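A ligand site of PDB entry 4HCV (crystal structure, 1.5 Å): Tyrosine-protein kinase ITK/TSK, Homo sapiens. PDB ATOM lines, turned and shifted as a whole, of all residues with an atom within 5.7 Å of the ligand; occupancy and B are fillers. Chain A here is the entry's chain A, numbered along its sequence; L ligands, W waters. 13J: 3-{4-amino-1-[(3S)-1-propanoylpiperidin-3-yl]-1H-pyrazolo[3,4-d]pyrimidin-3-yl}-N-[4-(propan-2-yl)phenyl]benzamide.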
ATOM      1  N   ILE A  18      32.274   3.497   2.067  1.00  0.00           N
ATOM      2  CA  ILE A  18      30.973   4.168   1.917  1.00  0.00           C
ATOM      3  C   ILE A  18      30.948   5.600   2.480  1.00  0.00           C
ATOM      4  O   ILE A  18      30.013   6.348   2.173  1.00  0.00           O
ATOM      5  CB  ILE A  18      29.797   3.289   2.427  1.00  0.00           C
ATOM      6  CG1 ILE A  18      29.933   2.960   3.944  1.00  0.00           C
ATOM      7  CG2 ILE A  18      29.661   2.049   1.534  1.00  0.00           C
ATOM      8  CD1 ILE A  18      28.664   2.233   4.571  1.00  0.00           C
ATOM      9  N   GLY A  19      31.907   5.949   3.326  1.00  0.00           N
ATOM     10  CA  GLY A  19      31.960   7.289   3.904  1.00  0.00           C
ATOM     11  C   GLY A  19      33.298   7.563   4.551  1.00  0.00           C
ATOM     12  O   GLY A  19      34.022   6.636   4.910  1.00  0.00           O
ATOM     13  N   SER A  20      33.651   8.831   4.672  1.00  0.00           N
ATOM     14  CA  SER A  20      34.885   9.221   5.318  1.00  0.00           C
ATOM     15  C   SER A  20      34.710  10.613   5.896  1.00  0.00           C
ATOM     16  O   SER A  20      33.897  11.397   5.399  1.00  0.00           O
ATOM     17  CB  SER A  20      36.054   9.228   4.335  1.00  0.00           C
ATOM     18  OG  SER A  20      35.904  10.248   3.373  1.00  0.00           O
ATOM     19  N   PHE A  23      37.793  11.915  11.754  1.00  0.00           N
ATOM     20  CA  PHE A  23      37.841  10.773  12.664  1.00  0.00           C
ATOM     21  C   PHE A  23      38.090   9.431  12.022  1.00  0.00           C
ATOM     22  O   PHE A  23      38.597   8.539  12.701  1.00  0.00           O
ATOM     23  CB  PHE A  23      36.724  10.744  13.731  1.00  0.00           C
ATOM     24  CG  PHE A  23      36.380  12.033  14.451  1.00  0.00           C
ATOM     25  CD1 PHE A  23      35.067  12.345  14.774  1.00  0.00           C
ATOM     26  CD2 PHE A  23      37.375  12.963  14.760  1.00  0.00           C
ATOM     27  CE1 PHE A  23      34.751  13.543  15.432  1.00  0.00           C
ATOM     28  CE2 PHE A  23      37.050  14.176  15.389  1.00  0.00           C
ATOM     29  CZ  PHE A  23      35.743  14.454  15.703  1.00  0.00           C
ATOM     30  N   VAL A  26      34.447   4.723   6.860  1.00  0.00           N
ATOM     31  CA  VAL A  26      33.439   3.688   7.062  1.00  0.00           C
ATOM     32  C   VAL A  26      33.422   2.818   5.801  1.00  0.00           C
ATOM     33  O   VAL A  26      33.295   3.331   4.689  1.00  0.00           O
ATOM     34  CB  VAL A  26      32.001   4.213   7.390  1.00  0.00           C
ATOM     35  CG1 VAL A  26      31.031   3.041   7.569  1.00  0.00           C
ATOM     36  CG2 VAL A  26      31.999   5.058   8.667  1.00  0.00           C
ATOM     37  N   ALA A  38      28.911  -2.519   8.909  1.00  0.00           N
ATOM     38  CA  ALA A  38      29.600  -1.259   8.633  1.00  0.00           C
ATOM     39  C   ALA A  38      30.796  -1.247   9.576  1.00  0.00           C
ATOM     40  O   ALA A  38      30.655  -1.470  10.783  1.00  0.00           O
ATOM     41  CB  ALA A  38      28.703  -0.059   8.908  1.00  0.00           C
ATOM     42  N   LYS A  40      33.969   0.969  11.017  1.00  0.00           N
ATOM     43  CA  LYS A  40      34.605   2.250  11.137  1.00  0.00           C
ATOM     44  C   LYS A  40      36.070   2.060  11.500  1.00  0.00           C
ATOM     45  O   LYS A  40      36.356   1.464  12.545  1.00  0.00           O
ATOM     46  CB  LYS A  40      33.898   3.089  12.223  1.00  0.00           C
ATOM     47  CG  LYS A  40      34.616   4.401  12.627  1.00  0.00           C
ATOM     48  CD  LYS A  40      34.581   5.475  11.513  1.00  0.00           C
ATOM     49  CE  LYS A  40      34.610   6.885  12.066  1.00  0.00           C
ATOM     50  NZ  LYS A  40      33.299   7.302  12.606  1.00  0.00           N
ATOM     51  N   ILE A  42      39.412   3.937  12.787  1.00  0.00           N
ATOM     52  CA  ILE A  42      39.701   5.157  13.533  1.00  0.00           C
ATOM     53  C   ILE A  42      41.099   5.688  13.246  1.00  0.00           C
ATOM     54  O   ILE A  42      42.085   4.984  13.434  1.00  0.00           O
ATOM     55  CB  ILE A  42      39.513   4.895  15.067  1.00  0.00           C
ATOM     56  CG1 ILE A  42      38.151   4.212  15.437  1.00  0.00           C
ATOM     57  CG2 ILE A  42      39.785   6.187  15.881  1.00  0.00           C
ATOM     58  CD1 ILE A  42      37.050   5.054  15.240  1.00  0.00           C
ATOM     59  N   ALA A  46      42.425  10.521  16.994  1.00  0.00           N
ATOM     60  CA  ALA A  46      41.048  11.049  16.922  1.00  0.00           C
ATOM     61  C   ALA A  46      40.237  10.707  18.160  1.00  0.00           C
ATOM     62  O   ALA A  46      39.337  11.449  18.543  1.00  0.00           O
ATOM     63  CB  ALA A  46      40.330  10.537  15.682  1.00  0.00           C
ATOM     64  N   MET A  47      40.520   9.552  18.761  1.00  0.00           N
ATOM     65  CA  MET A  47      39.756   9.121  19.940  1.00  0.00           C
ATOM     66  C   MET A  47      40.649   8.564  21.046  1.00  0.00           C
ATOM     67  O   MET A  47      41.774   8.117  20.795  1.00  0.00           O
ATOM     68  CB  MET A  47      38.670   8.093  19.561  1.00  0.00           C
ATOM     69  CG  MET A  47      39.153   6.682  19.519  1.00  0.00           C
ATOM     70  SD  MET A  47      37.908   5.494  18.935  1.00  0.00           S
ATOM     71  CE  MET A  47      36.754   5.543  20.140  1.00  0.00           C
ATOM     72  N   VAL A  68      21.314   1.559  16.775  1.00  0.00           N
ATOM     73  CA  VAL A  68      22.290   0.870  15.912  1.00  0.00           C
ATOM     74  C   VAL A  68      23.229   0.096  16.840  1.00  0.00           C
ATOM     75  O   VAL A  68      23.874   0.684  17.720  1.00  0.00           O
ATOM     76  CB  VAL A  68      23.054   1.878  15.029  1.00  0.00           C
ATOM     77  CG1 VAL A  68      24.123   1.171  14.176  1.00  0.00           C
ATOM     78  CG2 VAL A  68      22.110   2.664  14.131  1.00  0.00           C
ATOM     79  N   LEU A  82      35.788  -0.388  14.676  1.00  0.00           N
ATOM     80  CA  LEU A  82      34.547  -0.625  15.387  1.00  0.00           C
ATOM     81  C   LEU A  82      33.560  -1.202  14.396  1.00  0.00           C
ATOM     82  O   LEU A  82      33.467  -0.691  13.266  1.00  0.00           O
ATOM     83  CB  LEU A  82      33.976   0.638  15.999  1.00  0.00           C
ATOM     84  CG  LEU A  82      34.837   1.421  17.001  1.00  0.00           C
ATOM     85  CD1 LEU A  82      33.992   2.449  17.738  1.00  0.00           C
ATOM     86  CD2 LEU A  82      35.584   0.545  17.933  1.00  0.00           C
ATOM     87  N   PHE A  84      29.724  -2.310  13.306  1.00  0.00           N
ATOM     88  CA  PHE A  84      28.334  -1.960  13.567  1.00  0.00           C
ATOM     89  C   PHE A  84      27.381  -2.661  12.662  1.00  0.00           C
ATOM     90  O   PHE A  84      27.703  -3.086  11.539  1.00  0.00           O
ATOM     91  CB  PHE A  84      28.142  -0.456  13.316  1.00  0.00           C
ATOM     92  CG  PHE A  84      28.919   0.421  14.260  1.00  0.00           C
ATOM     93  CD1 PHE A  84      28.452   0.681  15.544  1.00  0.00           C
ATOM     94  CD2 PHE A  84      30.114   1.008  13.854  1.00  0.00           C
ATOM     95  CE1 PHE A  84      29.176   1.485  16.417  1.00  0.00           C
ATOM     96  CE2 PHE A  84      30.847   1.806  14.735  1.00  0.00           C
ATOM     97  CZ  PHE A  84      30.374   2.029  16.022  1.00  0.00           C
ATOM     98  N   GLU A  85      26.143  -2.759  13.150  1.00  0.00           N
ATOM     99  CA  GLU A  85      25.021  -3.183  12.371  1.00  0.00           C
ATOM    100  C   GLU A  85      24.957  -2.300  11.093  1.00  0.00           C
ATOM    101  O   GLU A  85      25.025  -1.077  11.176  1.00  0.00           O
ATOM    102  CB  GLU A  85      23.785  -2.933  13.256  1.00  0.00           C
ATOM    103  CG  GLU A  85      22.451  -3.081  12.556  1.00  0.00           C
ATOM    104  CD  GLU A  85      21.245  -2.790  13.412  1.00  0.00           C
ATOM    105  OE1 GLU A  85      21.406  -2.420  14.609  1.00  0.00           O
ATOM    106  OE2 GLU A  85      20.136  -2.997  12.905  1.00  0.00           O
ATOM    107  N   PHE A  86      24.848  -2.924   9.937  1.00  0.00           N
ATOM    108  CA  PHE A  86      24.776  -2.171   8.674  1.00  0.00           C
ATOM    109  C   PHE A  86      23.371  -1.609   8.473  1.00  0.00           C
ATOM    110  O   PHE A  86      22.391  -2.359   8.453  1.00  0.00           O
ATOM    111  CB  PHE A  86      25.177  -3.068   7.489  1.00  0.00           C
ATOM    112  CG  PHE A  86      25.179  -2.352   6.153  1.00  0.00           C
ATOM    113  CD1 PHE A  86      26.201  -1.477   5.824  1.00  0.00           C
ATOM    114  CD2 PHE A  86      24.152  -2.561   5.240  1.00  0.00           C
ATOM    115  CE1 PHE A  86      26.154  -0.746   4.612  1.00  0.00           C
ATOM    116  CE2 PHE A  86      24.146  -1.888   4.007  1.00  0.00           C
ATOM    117  CZ  PHE A  86      25.139  -0.984   3.713  1.00  0.00           C
ATOM    118  N   MET A  87      23.309  -0.283   8.228  1.00  0.00           N
ATOM    119  CA  MET A  87      22.034   0.433   7.993  1.00  0.00           C
ATOM    120  C   MET A  87      21.950   0.786   6.521  1.00  0.00           C
ATOM    121  O   MET A  87      22.686   1.659   6.051  1.00  0.00           O
ATOM    122  CB  MET A  87      21.957   1.670   8.882  1.00  0.00           C
ATOM    123  CG  MET A  87      22.057   1.301  10.398  1.00  0.00           C
ATOM    124  SD  MET A  87      20.692   0.254  10.942  1.00  0.00           S
ATOM    125  CE  MET A  87      19.321   1.380  10.711  1.00  0.00           C
ATOM    126  N   GLU A  88      21.124   0.022   5.789  1.00  0.00           N
ATOM    127  CA  GLU A  88      21.062   0.078   4.321  1.00  0.00           C
ATOM    128  C   GLU A  88      20.908   1.424   3.667  1.00  0.00           C
ATOM    129  O   GLU A  88      21.459   1.644   2.580  1.00  0.00           O
ATOM    130  CB  GLU A  88      20.140  -0.985   3.715  1.00  0.00           C
ATOM    131  CG  GLU A  88      18.675  -0.932   4.105  1.00  0.00           C
ATOM    132  CD  GLU A  88      17.832  -2.018   3.456  1.00  0.00           C
ATOM    133  OE1 GLU A  88      16.671  -1.728   3.088  1.00  0.00           O
ATOM    134  OE2 GLU A  88      18.340  -3.153   3.306  1.00  0.00           O
ATOM    135  N   GLY A  90      21.746   4.534   5.006  1.00  0.00           N
ATOM    136  CA  GLY A  90      22.660   5.564   5.465  1.00  0.00           C
ATOM    137  C   GLY A  90      22.051   6.514   6.480  1.00  0.00           C
ATOM    138  O   GLY A  90      21.126   6.148   7.210  1.00  0.00           O
ATOM    139  N   CYS A  91      22.659   7.677   6.601  1.00  0.00           N
ATOM    140  CA  CYS A  91      22.204   8.639   7.599  1.00  0.00           C
ATOM    141  C   CYS A  91      20.958   9.356   7.210  1.00  0.00           C
ATOM    142  O   CYS A  91      20.702   9.645   6.033  1.00  0.00           O
ATOM    143  CB  CYS A  91      23.312   9.624   7.927  1.00  0.00           C
ATOM    144  SG  CYS A  91      23.857  10.577   6.498  1.00  0.00           S
ATOM    145  N   LEU A  92      20.183   9.693   8.228  1.00  0.00           N
ATOM    146  CA  LEU A  92      18.915  10.377   8.047  1.00  0.00           C
ATOM    147  C   LEU A  92      19.076  11.758   7.434  1.00  0.00           C
ATOM    148  O   LEU A  92      18.249  12.130   6.605  1.00  0.00           O
ATOM    149  CB  LEU A  92      18.197  10.438   9.405  1.00  0.00           C
ATOM    150  CG  LEU A  92      16.818  11.073   9.414  1.00  0.00           C
ATOM    151  CD1 LEU A  92      15.822  10.342   8.472  1.00  0.00           C
ATOM    152  CD2 LEU A  92      16.278  11.107  10.833  1.00  0.00           C
ATOM    153  N   SER A  93      20.099  12.528   7.818  1.00  0.00           N
ATOM    154  CA  SER A  93      20.304  13.840   7.232  1.00  0.00           C
ATOM    155  C   SER A  93      20.381  13.801   5.715  1.00  0.00           C
ATOM    156  O   SER A  93      19.649  14.524   5.036  1.00  0.00           O
ATOM    157  CB  SER A  93      21.551  14.480   7.802  1.00  0.00           C
ATOM    158  OG  SER A  93      22.660  13.596   7.731  1.00  0.00           O
ATOM    159  N   ASP A  94      21.198  12.890   5.178  1.00  0.00           N
ATOM    160  CA  ASP A  94      21.333  12.795   3.734  1.00  0.00           C
ATOM    161  C   ASP A  94      20.116  12.157   3.089  1.00  0.00           C
ATOM    162  O   ASP A  94      19.763  12.515   1.979  1.00  0.00           O
ATOM    163  CB  ASP A  94      22.611  12.034   3.344  1.00  0.00           C
ATOM    164  CG  ASP A  94      23.897  12.828   3.554  1.00  0.00           C
ATOM    165  OD1 ASP A  94      23.815  14.073   3.771  1.00  0.00           O
ATOM    166  OD2 ASP A  94      24.970  12.214   3.539  1.00  0.00           O
ATOM    167  N   ARG A 135      22.255  13.691  11.452  1.00  0.00           N
ATOM    168  CA  ARG A 135      23.476  13.063  10.925  1.00  0.00           C
ATOM    169  C   ARG A 135      23.862  11.777  11.618  1.00  0.00           C
ATOM    170  O   ARG A 135      24.639  11.007  11.033  1.00  0.00           O
ATOM    171  CB  ARG A 135      24.676  14.010  10.959  1.00  0.00           C
ATOM    172  CG  ARG A 135      24.880  14.629  12.326  1.00  0.00           C
ATOM    173  CD  ARG A 135      26.021  15.653  12.283  1.00  0.00           C
ATOM    174  NE  ARG A 135      25.897  16.565  13.423  1.00  0.00           N
ATOM    175  CZ  ARG A 135      26.258  16.263  14.661  1.00  0.00           C
ATOM    176  NH1 ARG A 135      26.807  15.086  14.941  1.00  0.00           N
ATOM    177  NH2 ARG A 135      26.038  17.125  15.649  1.00  0.00           N
ATOM    178  N   LEU A 138      20.222   6.722  11.638  1.00  0.00           N
ATOM    179  CA  LEU A 138      20.435   5.935  10.412  1.00  0.00           C
ATOM    180  C   LEU A 138      19.152   5.303   9.960  1.00  0.00           C
ATOM    181  O   LEU A 138      18.257   5.043  10.753  1.00  0.00           O
ATOM    182  CB  LEU A 138      21.493   4.871  10.655  1.00  0.00           C
ATOM    183  CG  LEU A 138      22.914   5.444  10.789  1.00  0.00           C
ATOM    184  CD1 LEU A 138      23.690   4.758  11.805  1.00  0.00           C
ATOM    185  CD2 LEU A 138      23.657   5.367   9.490  1.00  0.00           C
ATOM    186  N   SER A 148      22.210   6.332  16.641  1.00  0.00           N
ATOM    187  CA  SER A 148      23.565   5.802  16.804  1.00  0.00           C
ATOM    188  C   SER A 148      24.416   6.835  17.513  1.00  0.00           C
ATOM    189  O   SER A 148      24.043   8.012  17.604  1.00  0.00           O
ATOM    190  CB  SER A 148      24.219   5.476  15.457  1.00  0.00           C
ATOM    191  OG  SER A 148      24.685   6.640  14.788  1.00  0.00           O
ATOM    192  N   ASP A 149      25.605   6.393  17.949  1.00  0.00           N
ATOM    193  CA  ASP A 149      26.615   7.300  18.479  1.00  0.00           C
ATOM    194  C   ASP A 149      26.333   7.912  19.839  1.00  0.00           C
ATOM    195  O   ASP A 149      27.030   8.849  20.249  1.00  0.00           O
ATOM    196  CB  ASP A 149      27.055   8.319  17.423  1.00  0.00           C
ATOM    197  CG  ASP A 149      27.929   7.691  16.354  1.00  0.00           C
ATOM    198  OD1 ASP A 149      28.409   6.567  16.573  1.00  0.00           O
ATOM    199  OD2 ASP A 149      28.177   8.361  15.350  1.00  0.00           O
ATOM    200  N   MET A 152      29.281   8.751  22.315  1.00  0.00           N
ATOM    201  CA  MET A 152      30.577   8.721  21.643  1.00  0.00           C
ATOM    202  C   MET A 152      31.419   9.991  21.750  1.00  0.00           C
ATOM    203  O   MET A 152      32.644   9.898  21.608  1.00  0.00           O
ATOM    204  CB  MET A 152      30.429   8.259  20.182  1.00  0.00           C
ATOM    205  CG  MET A 152      29.950   6.831  20.075  1.00  0.00           C
ATOM    206  SD  MET A 152      31.092   5.601  20.756  1.00  0.00           S
ATOM    207  CE  MET A 152      32.319   5.587  19.577  1.00  0.00           C
ATOM    208  N   THR A 153      30.797  11.180  21.949  1.00  0.00           N
ATOM    209  CA  THR A 153      31.632  12.391  22.079  1.00  0.00           C
ATOM    210  C   THR A 153      32.490  12.354  23.335  1.00  0.00           C
ATOM    211  O   THR A 153      33.444  13.151  23.442  1.00  0.00           O
ATOM    212  CB  THR A 153      30.823  13.687  21.987  1.00  0.00           C
ATOM    213  OG1 THR A 153      29.812  13.697  22.991  1.00  0.00           O
ATOM    214  CG2 THR A 153      30.229  13.895  20.591  1.00  0.00           C
ATOM    215  N   PHE A 155      34.613  10.201  23.870  1.00  0.00           N
ATOM    216  CA  PHE A 155      35.891   9.672  23.444  1.00  0.00           C
ATOM    217  C   PHE A 155      36.601  10.521  22.404  1.00  0.00           C
ATOM    218  O   PHE A 155      37.720  10.175  22.040  1.00  0.00           O
ATOM    219  CB  PHE A 155      35.729   8.228  22.929  1.00  0.00           C
ATOM    220  CG  PHE A 155      34.896   7.406  23.878  1.00  0.00           C
ATOM    221  CD1 PHE A 155      35.382   7.053  25.134  1.00  0.00           C
ATOM    222  CD2 PHE A 155      33.607   6.994  23.531  1.00  0.00           C
ATOM    223  CE1 PHE A 155      34.584   6.331  26.046  1.00  0.00           C
ATOM    224  CE2 PHE A 155      32.833   6.247  24.430  1.00  0.00           C
ATOM    225  CZ  PHE A 155      33.327   5.925  25.675  1.00  0.00           C
ATOM    226  N   VAL A 156      35.982  11.586  21.898  1.00  0.00           N
ATOM    227  CA  VAL A 156      36.601  12.457  20.914  1.00  0.00           C
ATOM    228  C   VAL A 156      37.727  13.246  21.583  1.00  0.00           C
ATOM    229  O   VAL A 156      37.487  13.844  22.631  1.00  0.00           O
ATOM    230  CB  VAL A 156      35.535  13.384  20.293  1.00  0.00           C
ATOM    231  CG1 VAL A 156      36.174  14.475  19.445  1.00  0.00           C
ATOM    232  CG2 VAL A 156      34.488  12.586  19.489  1.00  0.00           C
HETATM  233  C4  13J L   1      33.989   6.490  16.539  1.00  0.00           C
HETATM  234  C7  13J L   1      31.595   7.848  16.258  1.00  0.00           C
HETATM  235  C6  13J L   1      32.915   5.849  15.968  1.00  0.00           C
HETATM  236  C9  13J L   1      25.602   2.435   7.245  1.00  0.00           C
HETATM  237  C13 13J L   1      33.872   7.792  16.979  1.00  0.00           C
HETATM  238  C20 13J L   1      28.437   6.934   5.035  1.00  0.00           C
HETATM  239  C21 13J L   1      28.305   5.778   6.023  1.00  0.00           C
HETATM  240  C8  13J L   1      29.104   4.709  12.176  1.00  0.00           C
HETATM  241  C18 13J L   1      30.642   5.287  14.004  1.00  0.00           C
HETATM  242  C16 13J L   1      26.819   4.029   8.184  1.00  0.00           C
HETATM  243  C19 13J L   1      26.943   9.536   6.410  1.00  0.00           C
HETATM  244  C26 13J L   1      34.867   8.741  19.092  1.00  0.00           C
HETATM  245  C1  13J L   1      27.203   3.822  13.994  1.00  0.00           C
HETATM  246  C2  13J L   1      26.943   3.817  12.626  1.00  0.00           C
HETATM  247  C3  13J L   1      28.409   4.316  14.453  1.00  0.00           C
HETATM  248  C5  13J L   1      32.677   8.481  16.851  1.00  0.00           C
HETATM  249  C10 13J L   1      26.831   3.408   9.415  1.00  0.00           C
HETATM  250  C11 13J L   1      27.877   4.242  11.702  1.00  0.00           C
HETATM  251  C12 13J L   1      29.362   4.735  13.538  1.00  0.00           C
HETATM  252  C14 13J L   1      31.722   6.547  15.819  1.00  0.00           C
HETATM  253  C15 13J L   1      27.569   4.272  10.282  1.00  0.00           C
HETATM  254  C17 13J L   1      26.140   2.205   9.496  1.00  0.00           C
HETATM  255  C22 13J L   1      27.126   7.674   4.905  1.00  0.00           C
HETATM  256  C23 13J L   1      26.530   7.153   7.232  1.00  0.00           C
HETATM  257  C24 13J L   1      27.765   6.261   7.368  1.00  0.00           C
HETATM  258  C25 13J L   1      25.403  11.063   7.396  1.00  0.00           C
HETATM  259  C27 13J L   1      35.935   9.297  16.852  1.00  0.00           C
HETATM  260  C28 13J L   1      26.502  10.060   7.743  1.00  0.00           C
HETATM  261  C29 13J L   1      35.095   8.336  17.652  1.00  0.00           C
HETATM  262  N30 13J L   1      26.207   3.614   7.059  1.00  0.00           N
HETATM  263  N31 13J L   1      25.533   1.725   8.388  1.00  0.00           N
HETATM  264  N32 13J L   1      27.967   5.344   9.582  1.00  0.00           N
HETATM  265  N33 13J L   1      27.528   5.181   8.322  1.00  0.00           N
HETATM  266  N34 13J L   1      26.753   8.180   6.200  1.00  0.00           N
HETATM  267  N35 13J L   1      26.106   1.434  10.659  1.00  0.00           N
HETATM  268  N36 13J L   1      30.611   5.888  15.242  1.00  0.00           N
HETATM  269  O37 13J L   1      31.632   5.223  13.293  1.00  0.00           O
HETATM  270  O38 13J L   1      27.380  10.323   5.575  1.00  0.00           O
HETATM  271  O   HOH W   1      28.103  12.850   5.776  1.00  0.00           O
HETATM  272  O   HOH W   2      25.892   8.467  10.614  1.00  0.00           O
HETATM  273  O   HOH W   3      29.925   8.372  13.177  1.00  0.00           O
HETATM  274  O   HOH W   4      33.298   9.839  13.701  1.00  0.00           O
HETATM  275  O   HOH W   5      29.115   8.104  10.383  1.00  0.00           O
HETATM  276  O   HOH W   6      24.042   8.157   3.790  1.00  0.00           O
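The side-chain carboxylate (OD1) of Asp 149 lies within hydrogen-bond range of a nitrogen (N36) of the ligand. The side-chain sulfur (SG) of Cys 91 is bonded to a carbon (C25) of the ligand (1.9 Å). The backbone NH (N) of Met 87 lies within hydrogen-bond range of a nitrogen (N31) of the ligand (3.0 Å). The backbone carbonyl oxygen (O) of Glu 85 sits at hydrogen-bond distance from a nitrogen (N35) of the ligand, 2.8 Å away. NZ of Lys 40 sits at hydrogen-bond distance from O37 of the ligand (2.8 Å).
The backbone NH (N) of Lys 40 lies within hydrogen-bond range of the backbone carbonyl oxygen (O) of Leu 82 (2.8 Å). The backbone carbonyl oxygen of Ala 38 sits at hydrogen-bond distance from the backbone NH of Phe 84 (2.8 Å). The backbone carbonyl oxygen (O) of Gly 19 lies within hydrogen-bond range of the backbone NH (N) of Val 26. The side-chain hydroxyl (OG) of Ser 93 sits at hydrogen-bond distance from the side-chain sulfur (SG) of Cys 91, 3.5 Å away. The side-chain sulfur (SG) of Cys 91 sits close to the backbone NH (N) of Asp 94, 3.8 Å away. N of Ile 18 lies within hydrogen-bond range of O of Val 26 (2.8 Å).
O of Ile 18 touches C20 of the ligand, 3.3 Å away. CA of Gly 19 touches C20 of the ligand, at 3.7 Å. CB of Phe 23 touches C27 of the ligand, 3.5 Å away. Ala 38 touches the ligand (CB to N35, 3.5 Å). Ile 42 touches the ligand. Met 47 touches the ligand (CE to C26, 3.9 Å). CD1 of Leu 82 touches C6 of the ligand (3.98 Å). CZ of Phe 84 touches C3 of the ligand (3.4 Å). C of Phe 86 touches N31 of the ligand, at 3.97 Å. Ser 93 touches the ligand. Asp 94 touches the ligand (OD2 to O38, 3.7 Å). Arg 135 touches the ligand. Leu 138 touches the ligand. CB of Ser 148 touches C1 of the ligand, 3.7 Å away. Met 152 touches the ligand. Phe 155 touches the ligand (CB to C26, 3.97 Å). Val 156 touches the ligand. Hydrophobic or aromatic side chains that line the ligand: Ile 18, Phe 23, Ala 38, Ile 42, Met 47, Leu 82, Phe 84, Met 87, Leu 138, Met 152, Phe 155 and Val 156. Within 4 Å of the ligand: Ile 18, Gly 19, Phe 23, Ala 38, Lys 40, Ile 42, Met 47, Leu 82, Phe 84, Glu 85, Phe 86, Met 87, Cys 91, Ser 93, Asp 94, Arg 135, Leu 138, Ser 148, Asp 149, Met 152, Phe 155 and Val 156. The nearest printed residue that does not touch the ligand is Val 68 (4.05 Å).
Water W3 lies within hydrogen-bond range of OD2 of Asp 149 and N36 of the ligand.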
